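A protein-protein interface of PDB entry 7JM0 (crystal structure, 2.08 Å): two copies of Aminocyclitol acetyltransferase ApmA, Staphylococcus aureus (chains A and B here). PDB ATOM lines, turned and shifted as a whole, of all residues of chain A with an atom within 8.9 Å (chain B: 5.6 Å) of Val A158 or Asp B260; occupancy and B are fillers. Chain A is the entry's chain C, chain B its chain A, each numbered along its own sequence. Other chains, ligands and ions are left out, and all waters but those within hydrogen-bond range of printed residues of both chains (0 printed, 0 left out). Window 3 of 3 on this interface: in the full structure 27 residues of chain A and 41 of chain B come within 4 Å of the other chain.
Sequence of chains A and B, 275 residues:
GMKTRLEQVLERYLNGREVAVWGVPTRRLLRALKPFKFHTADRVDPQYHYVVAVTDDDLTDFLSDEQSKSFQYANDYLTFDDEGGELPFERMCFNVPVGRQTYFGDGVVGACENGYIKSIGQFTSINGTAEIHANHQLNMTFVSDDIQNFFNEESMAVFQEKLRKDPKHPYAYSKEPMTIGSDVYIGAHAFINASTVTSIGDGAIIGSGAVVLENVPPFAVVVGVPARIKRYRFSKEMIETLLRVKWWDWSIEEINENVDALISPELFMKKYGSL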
ATOM      1  N   ASN A 139      27.571  16.776  -2.684  1.00  0.00           N
ATOM      2  CA  ASN A 139      27.585  15.415  -2.159  1.00  0.00           C
ATOM      3  C   ASN A 139      26.581  14.516  -2.875  1.00  0.00           C
ATOM      4  O   ASN A 139      26.105  13.529  -2.311  1.00  0.00           O
ATOM      5  CB  ASN A 139      27.331  15.419  -0.653  1.00  0.00           C
ATOM      6  CG  ASN A 139      28.449  16.092   0.121  1.00  0.00           C
ATOM      7  OD1 ASN A 139      28.533  17.318   0.170  1.00  0.00           O
ATOM      8  ND2 ASN A 139      29.314  15.289   0.732  1.00  0.00           N
ATOM      9  N   MET A 140      26.244  14.844  -4.114  1.00  0.00           N
ATOM     10  CA  MET A 140      25.477  13.944  -4.961  1.00  0.00           C
ATOM     11  C   MET A 140      26.411  13.268  -5.958  1.00  0.00           C
ATOM     12  O   MET A 140      27.595  13.593  -6.057  1.00  0.00           O
ATOM     13  CB  MET A 140      24.355  14.698  -5.679  1.00  0.00           C
ATOM     14  CG  MET A 140      23.340  15.325  -4.731  1.00  0.00           C
ATOM     15  SD  MET A 140      21.891  15.985  -5.582  1.00  0.00           S
ATOM     16  CE  MET A 140      21.007  16.719  -4.203  1.00  0.00           C
ATOM     17  N   THR A 141      25.864  12.299  -6.695  1.00  0.00           N
ATOM     18  CA  THR A 141      26.668  11.633  -7.714  1.00  0.00           C
ATOM     19  C   THR A 141      27.066  12.605  -8.819  1.00  0.00           C
ATOM     20  O   THR A 141      28.124  12.444  -9.439  1.00  0.00           O
ATOM     21  CB  THR A 141      25.905  10.432  -8.283  1.00  0.00           C
ATOM     22  OG1 THR A 141      25.480   9.585  -7.207  1.00  0.00           O
ATOM     23  CG2 THR A 141      26.777   9.627  -9.241  1.00  0.00           C
ATOM     24  N   PHE A 142      26.254  13.634  -9.054  1.00  0.00           N
ATOM     25  CA  PHE A 142      26.537  14.648 -10.055  1.00  0.00           C
ATOM     26  C   PHE A 142      26.708  16.003  -9.388  1.00  0.00           C
ATOM     27  O   PHE A 142      26.151  16.267  -8.318  1.00  0.00           O
ATOM     28  CB  PHE A 142      25.417  14.733 -11.110  1.00  0.00           C
ATOM     29  CG  PHE A 142      24.075  15.096 -10.544  1.00  0.00           C
ATOM     30  CD1 PHE A 142      23.250  14.122 -10.001  1.00  0.00           C
ATOM     31  CD2 PHE A 142      23.633  16.408 -10.560  1.00  0.00           C
ATOM     32  CE1 PHE A 142      22.009  14.452  -9.478  1.00  0.00           C
ATOM     33  CE2 PHE A 142      22.393  16.745 -10.039  1.00  0.00           C
ATOM     34  CZ  PHE A 142      21.581  15.765  -9.498  1.00  0.00           C
ATOM     35  N   PHE A 151      15.061  16.658 -15.984  1.00  0.00           N
ATOM     36  CA  PHE A 151      14.229  16.022 -14.972  1.00  0.00           C
ATOM     37  C   PHE A 151      12.758  16.314 -15.247  1.00  0.00           C
ATOM     38  O   PHE A 151      12.378  17.470 -15.459  1.00  0.00           O
ATOM     39  CB  PHE A 151      14.600  16.520 -13.573  1.00  0.00           C
ATOM     40  CG  PHE A 151      15.922  16.008 -13.064  1.00  0.00           C
ATOM     41  CD1 PHE A 151      16.532  14.906 -13.643  1.00  0.00           C
ATOM     42  CD2 PHE A 151      16.551  16.628 -11.994  1.00  0.00           C
ATOM     43  CE1 PHE A 151      17.751  14.437 -13.168  1.00  0.00           C
ATOM     44  CE2 PHE A 151      17.765  16.167 -11.517  1.00  0.00           C
ATOM     45  CZ  PHE A 151      18.367  15.071 -12.104  1.00  0.00           C
ATOM     46  N   ASN A 152      11.928  15.274 -15.230  1.00  0.00           N
ATOM     47  CA  ASN A 152      10.488  15.484 -15.313  1.00  0.00           C
ATOM     48  C   ASN A 152       9.993  15.980 -13.954  1.00  0.00           C
ATOM     49  O   ASN A 152      10.780  16.254 -13.043  1.00  0.00           O
ATOM     50  CB  ASN A 152       9.776  14.215 -15.786  1.00  0.00           C
ATOM     51  CG  ASN A 152      10.048  13.009 -14.902  1.00  0.00           C
ATOM     52  OD1 ASN A 152      10.161  13.123 -13.683  1.00  0.00           O
ATOM     53  ND2 ASN A 152      10.137  11.837 -15.520  1.00  0.00           N
ATOM     54  N   GLU A 153       8.672  16.095 -13.802  1.00  0.00           N
ATOM     55  CA  GLU A 153       8.116  16.686 -12.589  1.00  0.00           C
ATOM     56  C   GLU A 153       8.468  15.866 -11.352  1.00  0.00           C
ATOM     57  O   GLU A 153       8.857  16.426 -10.321  1.00  0.00           O
ATOM     58  CB  GLU A 153       6.599  16.831 -12.727  1.00  0.00           C
ATOM     59  CG  GLU A 153       5.909  17.348 -11.475  1.00  0.00           C
ATOM     60  CD  GLU A 153       4.501  17.842 -11.750  1.00  0.00           C
ATOM     61  OE1 GLU A 153       4.105  18.869 -11.157  1.00  0.00           O
ATOM     62  OE2 GLU A 153       3.792  17.206 -12.560  1.00  0.00           O
ATOM     63  N   GLU A 154       8.346  14.540 -11.436  1.00  0.00           N
ATOM     64  CA  GLU A 154       8.643  13.693 -10.284  1.00  0.00           C
ATOM     65  C   GLU A 154      10.117  13.777  -9.904  1.00  0.00           C
ATOM     66  O   GLU A 154      10.453  14.000  -8.734  1.00  0.00           O
ATOM     67  CB  GLU A 154       8.244  12.247 -10.579  1.00  0.00           C
ATOM     68  CG  GLU A 154       8.044  11.372  -9.344  1.00  0.00           C
ATOM     69  CD  GLU A 154       9.351  10.911  -8.717  1.00  0.00           C
ATOM     70  OE1 GLU A 154       9.375  10.682  -7.489  1.00  0.00           O
ATOM     71  OE2 GLU A 154      10.355  10.784  -9.449  1.00  0.00           O
ATOM     72  N   SER A 155      11.011  13.597 -10.882  1.00  0.00           N
ATOM     73  CA  SER A 155      12.442  13.613 -10.587  1.00  0.00           C
ATOM     74  C   SER A 155      12.883  14.967 -10.047  1.00  0.00           C
ATOM     75  O   SER A 155      13.695  15.040  -9.118  1.00  0.00           O
ATOM     76  CB  SER A 155      13.238  13.250 -11.838  1.00  0.00           C
ATOM     77  OG  SER A 155      13.015  11.899 -12.208  1.00  0.00           O
ATOM     78  N   MET A 156      12.354  16.055 -10.612  1.00  0.00           N
ATOM     79  CA  MET A 156      12.709  17.382 -10.119  1.00  0.00           C
ATOM     80  C   MET A 156      12.267  17.569  -8.674  1.00  0.00           C
ATOM     81  O   MET A 156      13.009  18.132  -7.861  1.00  0.00           O
ATOM     82  CB  MET A 156      12.092  18.463 -11.006  1.00  0.00           C
ATOM     83  CG  MET A 156      12.353  19.876 -10.496  1.00  0.00           C
ATOM     84  SD  MET A 156      14.084  20.361 -10.689  1.00  0.00           S
ATOM     85  CE  MET A 156      14.099  20.838 -12.409  1.00  0.00           C
ATOM     86  N   ALA A 157      11.063  17.101  -8.335  1.00  0.00           N
ATOM     87  CA  ALA A 157      10.574  17.243  -6.966  1.00  0.00           C
ATOM     88  C   ALA A 157      11.462  16.490  -5.983  1.00  0.00           C
ATOM     89  O   ALA A 157      11.701  16.962  -4.863  1.00  0.00           O
ATOM     90  CB  ALA A 157       9.128  16.759  -6.870  1.00  0.00           C
ATOM     91  N   VAL A 158      11.956  15.315  -6.381  1.00  0.00           N
ATOM     92  CA  VAL A 158      12.903  14.591  -5.538  1.00  0.00           C
ATOM     93  C   VAL A 158      14.200  15.378  -5.409  1.00  0.00           C
ATOM     94  O   VAL A 158      14.747  15.530  -4.310  1.00  0.00           O
ATOM     95  CB  VAL A 158      13.154  13.182  -6.101  1.00  0.00           C
ATOM     96  CG1 VAL A 158      14.094  12.408  -5.189  1.00  0.00           C
ATOM     97  CG2 VAL A 158      11.843  12.443  -6.267  1.00  0.00           C
ATOM     98  N   PHE A 159      14.701  15.899  -6.533  1.00  0.00           N
ATOM     99  CA  PHE A 159      15.927  16.691  -6.522  1.00  0.00           C
ATOM    100  C   PHE A 159      15.775  17.932  -5.647  1.00  0.00           C
ATOM    101  O   PHE A 159      16.648  18.237  -4.826  1.00  0.00           O
ATOM    102  CB  PHE A 159      16.298  17.077  -7.953  1.00  0.00           C
ATOM    103  CG  PHE A 159      17.560  17.885  -8.064  1.00  0.00           C
ATOM    104  CD1 PHE A 159      18.739  17.444  -7.485  1.00  0.00           C
ATOM    105  CD2 PHE A 159      17.572  19.075  -8.776  1.00  0.00           C
ATOM    106  CE1 PHE A 159      19.905  18.187  -7.597  1.00  0.00           C
ATOM    107  CE2 PHE A 159      18.732  19.819  -8.894  1.00  0.00           C
ATOM    108  CZ  PHE A 159      19.902  19.376  -8.302  1.00  0.00           C
ATOM    109  N   GLN A 160      14.663  18.656  -5.805  1.00  0.00           N
ATOM    110  CA  GLN A 160      14.465  19.887  -5.046  1.00  0.00           C
ATOM    111  C   GLN A 160      14.356  19.609  -3.551  1.00  0.00           C
ATOM    112  O   GLN A 160      14.872  20.379  -2.732  1.00  0.00           O
ATOM    113  CB  GLN A 160      13.218  20.617  -5.547  1.00  0.00           C
ATOM    114  CG  GLN A 160      13.364  21.192  -6.946  1.00  0.00           C
ATOM    115  CD  GLN A 160      14.467  22.230  -7.034  1.00  0.00           C
ATOM    116  OE1 GLN A 160      14.703  22.978  -6.086  1.00  0.00           O
ATOM    117  NE2 GLN A 160      15.155  22.271  -8.170  1.00  0.00           N
ATOM    118  N   GLU A 161      13.693  18.512  -3.179  1.00  0.00           N
ATOM    119  CA  GLU A 161      13.520  18.199  -1.763  1.00  0.00           C
ATOM    120  C   GLU A 161      14.858  17.909  -1.093  1.00  0.00           C
ATOM    121  O   GLU A 161      15.116  18.380   0.021  1.00  0.00           O
ATOM    122  CB  GLU A 161      12.564  17.016  -1.605  1.00  0.00           C
ATOM    123  CG  GLU A 161      11.839  16.968  -0.271  1.00  0.00           C
ATOM    124  CD  GLU A 161      12.719  16.465   0.856  1.00  0.00           C
ATOM    125  OE1 GLU A 161      13.391  15.429   0.667  1.00  0.00           O
ATOM    126  OE2 GLU A 161      12.739  17.104   1.929  1.00  0.00           O
ATOM    127  N   LYS A 162      15.723  17.135  -1.751  1.00  0.00           N
ATOM    128  CA  LYS A 162      17.007  16.811  -1.141  1.00  0.00           C
ATOM    129  C   LYS A 162      17.958  18.001  -1.166  1.00  0.00           C
ATOM    130  O   LYS A 162      18.835  18.106  -0.300  1.00  0.00           O
ATOM    131  CB  LYS A 162      17.623  15.593  -1.829  1.00  0.00           C
ATOM    132  CG  LYS A 162      16.833  14.311  -1.586  1.00  0.00           C
ATOM    133  CD  LYS A 162      17.532  13.413  -0.569  1.00  0.00           C
ATOM    134  CE  LYS A 162      16.746  12.133  -0.314  1.00  0.00           C
ATOM    135  NZ  LYS A 162      15.592  12.351   0.605  1.00  0.00           N
ATOM    136  N   LEU A 163      17.805  18.906  -2.139  1.00  0.00           N
ATOM    137  CA  LEU A 163      18.558  20.156  -2.101  1.00  0.00           C
ATOM    138  C   LEU A 163      18.195  20.968  -0.866  1.00  0.00           C
ATOM    139  O   LEU A 163      19.068  21.553  -0.215  1.00  0.00           O
ATOM    140  CB  LEU A 163      18.297  20.976  -3.361  1.00  0.00           C
ATOM    141  CG  LEU A 163      18.966  20.551  -4.669  1.00  0.00           C
ATOM    142  CD1 LEU A 163      18.554  21.494  -5.797  1.00  0.00           C
ATOM    143  CD2 LEU A 163      20.477  20.519  -4.516  1.00  0.00           C
ATOM    144  N   ARG A 164      16.907  21.006  -0.523  1.00  0.00           N
ATOM    145  CA  ARG A 164      16.464  21.764   0.638  1.00  0.00           C
ATOM    146  C   ARG A 164      16.967  21.179   1.953  1.00  0.00           C
ATOM    147  O   ARG A 164      17.047  21.916   2.943  1.00  0.00           O
ATOM    148  CB  ARG A 164      14.939  21.838   0.672  1.00  0.00           C
ATOM    149  CG  ARG A 164      14.331  22.848  -0.284  1.00  0.00           C
ATOM    150  CD  ARG A 164      12.837  22.992  -0.044  1.00  0.00           C
ATOM    151  NE  ARG A 164      12.114  21.782  -0.419  1.00  0.00           N
ATOM    152  CZ  ARG A 164      11.571  21.577  -1.615  1.00  0.00           C
ATOM    153  NH1 ARG A 164      11.669  22.504  -2.556  1.00  0.00           N
ATOM    154  NH2 ARG A 164      10.931  20.443  -1.867  1.00  0.00           N
ATOM    155  N   LYS A 165      17.336  19.901   1.955  1.00  0.00           N
ATOM    156  CA  LYS A 165      17.825  19.246   3.164  1.00  0.00           C
ATOM    157  C   LYS A 165      19.351  19.239   3.279  1.00  0.00           C
ATOM    158  O   LYS A 165      19.899  18.751   4.268  1.00  0.00           O
ATOM    159  CB  LYS A 165      17.290  17.814   3.247  1.00  0.00           C
ATOM    160  CG  LYS A 165      17.829  16.886   2.169  1.00  0.00           C
ATOM    161  CD  LYS A 165      19.080  16.162   2.640  1.00  0.00           C
ATOM    162  CE  LYS A 165      20.193  16.255   1.609  1.00  0.00           C
ATOM    163  NZ  LYS A 165      21.517  16.510   2.242  1.00  0.00           N
ATOM    164  N   ASN B 256      16.161  10.007 -15.769  1.00  0.00           N
ATOM    165  CA  ASN B 256      14.998  10.116 -14.891  1.00  0.00           C
ATOM    166  C   ASN B 256      14.781   8.833 -14.099  1.00  0.00           C
ATOM    167  O   ASN B 256      14.458   8.879 -12.906  1.00  0.00           O
ATOM    168  CB  ASN B 256      13.751  10.463 -15.707  1.00  0.00           C
ATOM    169  CG  ASN B 256      13.623  11.950 -15.969  1.00  0.00           C
ATOM    170  OD1 ASN B 256      13.193  12.712 -15.098  1.00  0.00           O
ATOM    171  ND2 ASN B 256      14.001  12.375 -17.171  1.00  0.00           N
ATOM    172  N   ASN B 258      16.957   6.910 -13.023  1.00  0.00           N
ATOM    173  CA  ASN B 258      18.055   6.737 -12.079  1.00  0.00           C
ATOM    174  C   ASN B 258      18.223   7.947 -11.167  1.00  0.00           C
ATOM    175  O   ASN B 258      19.317   8.165 -10.640  1.00  0.00           O
ATOM    176  CB  ASN B 258      19.368   6.469 -12.818  1.00  0.00           C
ATOM    177  CG  ASN B 258      19.458   5.064 -13.370  1.00  0.00           C
ATOM    178  OD1 ASN B 258      20.027   4.173 -12.738  1.00  0.00           O
ATOM    179  ND2 ASN B 258      18.902   4.858 -14.563  1.00  0.00           N
ATOM    180  N   VAL B 259      17.165   8.739 -10.970  1.00  0.00           N
ATOM    181  CA  VAL B 259      17.315  10.006 -10.259  1.00  0.00           C
ATOM    182  C   VAL B 259      17.751   9.771  -8.816  1.00  0.00           C
ATOM    183  O   VAL B 259      18.584  10.512  -8.280  1.00  0.00           O
ATOM    184  CB  VAL B 259      16.018  10.836 -10.344  1.00  0.00           C
ATOM    185  CG1 VAL B 259      14.869  10.158  -9.605  1.00  0.00           C
ATOM    186  CG2 VAL B 259      16.254  12.238  -9.809  1.00  0.00           C
ATOM    187  N   ASP B 260      17.219   8.727  -8.171  1.00  0.00           N
ATOM    188  CA  ASP B 260      17.641   8.425  -6.805  1.00  0.00           C
ATOM    189  C   ASP B 260      19.114   8.040  -6.759  1.00  0.00           C
ATOM    190  O   ASP B 260      19.844   8.448  -5.847  1.00  0.00           O
ATOM    191  CB  ASP B 260      16.781   7.306  -6.213  1.00  0.00           C
ATOM    192  CG  ASP B 260      15.391   7.776  -5.823  1.00  0.00           C
ATOM    193  OD1 ASP B 260      15.077   8.968  -6.019  1.00  0.00           O
ATOM    194  OD2 ASP B 260      14.609   6.947  -5.317  1.00  0.00           O
ATOM    195  N   ALA B 261      19.569   7.252  -7.737  1.00  0.00           N
ATOM    196  CA  ALA B 261      20.971   6.854  -7.778  1.00  0.00           C
ATOM    197  C   ALA B 261      21.870   8.041  -8.101  1.00  0.00           C
ATOM    198  O   ALA B 261      22.995   8.132  -7.595  1.00  0.00           O
ATOM    199  CB  ALA B 261      21.165   5.733  -8.797  1.00  0.00           C
ATOM    200  N   LEU B 262      21.391   8.962  -8.942  1.00  0.00           N
ATOM    201  CA  LEU B 262      22.175  10.153  -9.240  1.00  0.00           C
ATOM    202  C   LEU B 262      22.202  11.114  -8.057  1.00  0.00           C
ATOM    203  O   LEU B 262      23.175  11.853  -7.886  1.00  0.00           O
ATOM    204  CB  LEU B 262      21.625  10.845 -10.486  1.00  0.00           C
ATOM    205  CG  LEU B 262      21.842  10.076 -11.795  1.00  0.00           C
ATOM    206  CD1 LEU B 262      20.977  10.637 -12.921  1.00  0.00           C
ATOM    207  CD2 LEU B 262      23.314  10.098 -12.184  1.00  0.00           C
ATOM    208  N   ILE B 263      21.159  11.113  -7.227  1.00  0.00           N
ATOM    209  CA  ILE B 263      21.164  11.975  -6.050  1.00  0.00           C
ATOM    210  C   ILE B 263      22.029  11.380  -4.946  1.00  0.00           C
ATOM    211  O   ILE B 263      22.813  12.089  -4.308  1.00  0.00           O
ATOM    212  CB  ILE B 263      19.722  12.229  -5.569  1.00  0.00           C
ATOM    213  CG1 ILE B 263      19.002  13.178  -6.530  1.00  0.00           C
ATOM    214  CG2 ILE B 263      19.720  12.798  -4.160  1.00  0.00           C
ATOM    215  CD1 ILE B 263      17.536  13.380  -6.199  1.00  0.00           C
ATOM    216  N   SER B 264      21.918  10.075  -4.708  1.00  0.00           N
ATOM    217  CA  SER B 264      22.596   9.448  -3.579  1.00  0.00           C
ATOM    218  C   SER B 264      23.758   8.595  -4.067  1.00  0.00           C
ATOM    219  O   SER B 264      23.530   7.550  -4.697  1.00  0.00           O
ATOM    220  CB  SER B 264      21.613   8.600  -2.768  1.00  0.00           C
ATOM    221  OG  SER B 264      22.306   7.740  -1.873  1.00  0.00           O
ATOM    222  N   PRO B 265      25.007   8.990  -3.804  1.00  0.00           N
ATOM    223  CA  PRO B 265      26.140   8.130  -4.186  1.00  0.00           C
ATOM    224  C   PRO B 265      26.079   6.747  -3.564  1.00  0.00           C
ATOM    225  O   PRO B 265      26.508   5.775  -4.200  1.00  0.00           O
ATOM    226  CB  PRO B 265      27.362   8.919  -3.690  1.00  0.00           C
ATOM    227  CG  PRO B 265      26.895  10.343  -3.649  1.00  0.00           C
ATOM    228  CD  PRO B 265      25.451  10.278  -3.243  1.00  0.00           C
ATOM    229  N   LEU B 267      23.385   4.950  -2.986  1.00  0.00           N
ATOM    230  CA  LEU B 267      22.481   4.143  -3.798  1.00  0.00           C
ATOM    231  C   LEU B 267      23.079   3.837  -5.167  1.00  0.00           C
ATOM    232  O   LEU B 267      22.815   2.769  -5.729  1.00  0.00           O
ATOM    233  CB  LEU B 267      21.130   4.844  -3.954  1.00  0.00           C
ATOM    234  CG  LEU B 267      20.364   5.137  -2.662  1.00  0.00           C
ATOM    235  CD1 LEU B 267      19.103   5.946  -2.952  1.00  0.00           C
ATOM    236  CD2 LEU B 267      20.025   3.849  -1.917  1.00  0.00           C
ATOM    237  N   PHE B 268      23.877   4.754  -5.717  1.00  0.00           N
ATOM    238  CA  PHE B 268      24.538   4.490  -6.990  1.00  0.00           C
ATOM    239  C   PHE B 268      25.448   3.272  -6.885  1.00  0.00           C
ATOM    240  O   PHE B 268      25.439   2.397  -7.760  1.00  0.00           O
ATOM    241  CB  PHE B 268      25.327   5.720  -7.441  1.00  0.00           C
ATOM    242  CG  PHE B 268      25.963   5.573  -8.798  1.00  0.00           C
ATOM    243  CD1 PHE B 268      27.218   4.999  -8.936  1.00  0.00           C
ATOM    244  CD2 PHE B 268      25.305   6.012  -9.935  1.00  0.00           C
ATOM    245  CE1 PHE B 268      27.801   4.860 -10.186  1.00  0.00           C
ATOM    246  CE2 PHE B 268      25.882   5.878 -11.182  1.00  0.00           C
ATOM    247  CZ  PHE B 268      27.132   5.300 -11.309  1.00  0.00           C
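Among the printed residues, pairs that only touch across the chains: Asn A139 with Pro B265 (3.4 Å), Met A140 with Leu B262 (3.8 Å), Met A140 with Ile B263 (3.3 Å), Met A140 with Pro B265 (3.8 Å), Thr A141 with Ile B263 (3.9 Å), Thr A141 with Ser B264 (3.7 Å), Thr A141 with Phe B268 (3.9 Å), Phe A142 with Leu B262 (3.1 Å), Phe A151 with Asn B256 (3.5 Å), Ser A155 with Val B259 (3.6 Å), Val A158 with Asp B260 (3.7 Å), Val A158 with Ile B263 (3.7 Å) and Phe A159 with Ile B263 (3.7 Å).
Printed residues of chain B within 4 Å of Phe A151: Asn B256.
Of the printed residues of chain B, Asn A152 touches Asn B256.
Val A158 touches two residues of chain B.
Printed residues of chain B within 4 Å of Phe A159: Ile B263 (3.7 Å).
Gln A160 touches none of the printed residues of chain B.
Arg A164 touches none of the printed residues of chain B.
Of the printed residues of chain A, Asn B256 touches Phe A151 (3.5 Å), Asn A152 (2.9 Å) and Ser A155 (3.0 Å).
Of chain A, only Ser A155 comes within 4 Å of Val B259.
Of chain A, only Val A158 comes within 4 Å of Asp B260.
Of chain A, only Thr A141 (2.9 Å) comes within 4 Å of Ala B261.
Printed residues of chain A within 4 Å of Ile B263: Met A140, Thr A141, Val A158 and Phe A159.
Ser B264 touches one residue of chain A.
The nearest residue of chain A that does not touch Asp B260 is Thr A141 (5.9 Å).
The nearest printed residue of chain B that does not touch Asn A152 is Val B259 (6.9 Å).
O of Ala B261 is in hydrogen-bond range of OG1 of Thr A141 (2.9 Å).
OD1 of Asn B256 lies within hydrogen-bond range of OG of Ser A155 (3.0 Å).
The side-chain amide oxygen of Asn B256 sits at hydrogen-bond distance from the backbone NH of Asn A152 (2.9 Å).
The side-chain hydroxyl of Thr A141 sits close to the backbone nitrogen of Pro B265 (3.5 Å).
N of Thr A141 lies within hydrogen-bond range of O of Leu B262 (3.0 Å).
The side-chain amide oxygen of Asn A152 is in hydrogen-bond range of the backbone NH of Ser A155 (3.0 Å).
N of Leu B267 sits at hydrogen-bond distance from OG of Ser B264 (3.2 Å).
The side-chain amide oxygen (OD1) of Asn A152 lies within hydrogen-bond range of the backbone NH (N) of Glu A154 (3.2 Å).
Of the 11 printed residues of chain B, 9 touch a printed residue of chain A.
Hydrophobic or aromatic side chains of chain B within 4 Å of the printed part of chain A: Val B259, Leu B262, Ile B263, Pro B265 and Phe B268.
Along chain B the printed residues that touch a printed residue of chain A span positions 256 to 268.
Hydrophobic or aromatic side chains of chain A within 4 Å of the printed part of chain B: Met A140, Phe A142 and Val A158.
Among the printed residues, 18 pairs touch across the chains.
Among the printed residues, no Asp or Glu carboxylate lies within 4 Å of a Lys or Arg side-chain nitrogen of the other chain.
No position is printed for both chains.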
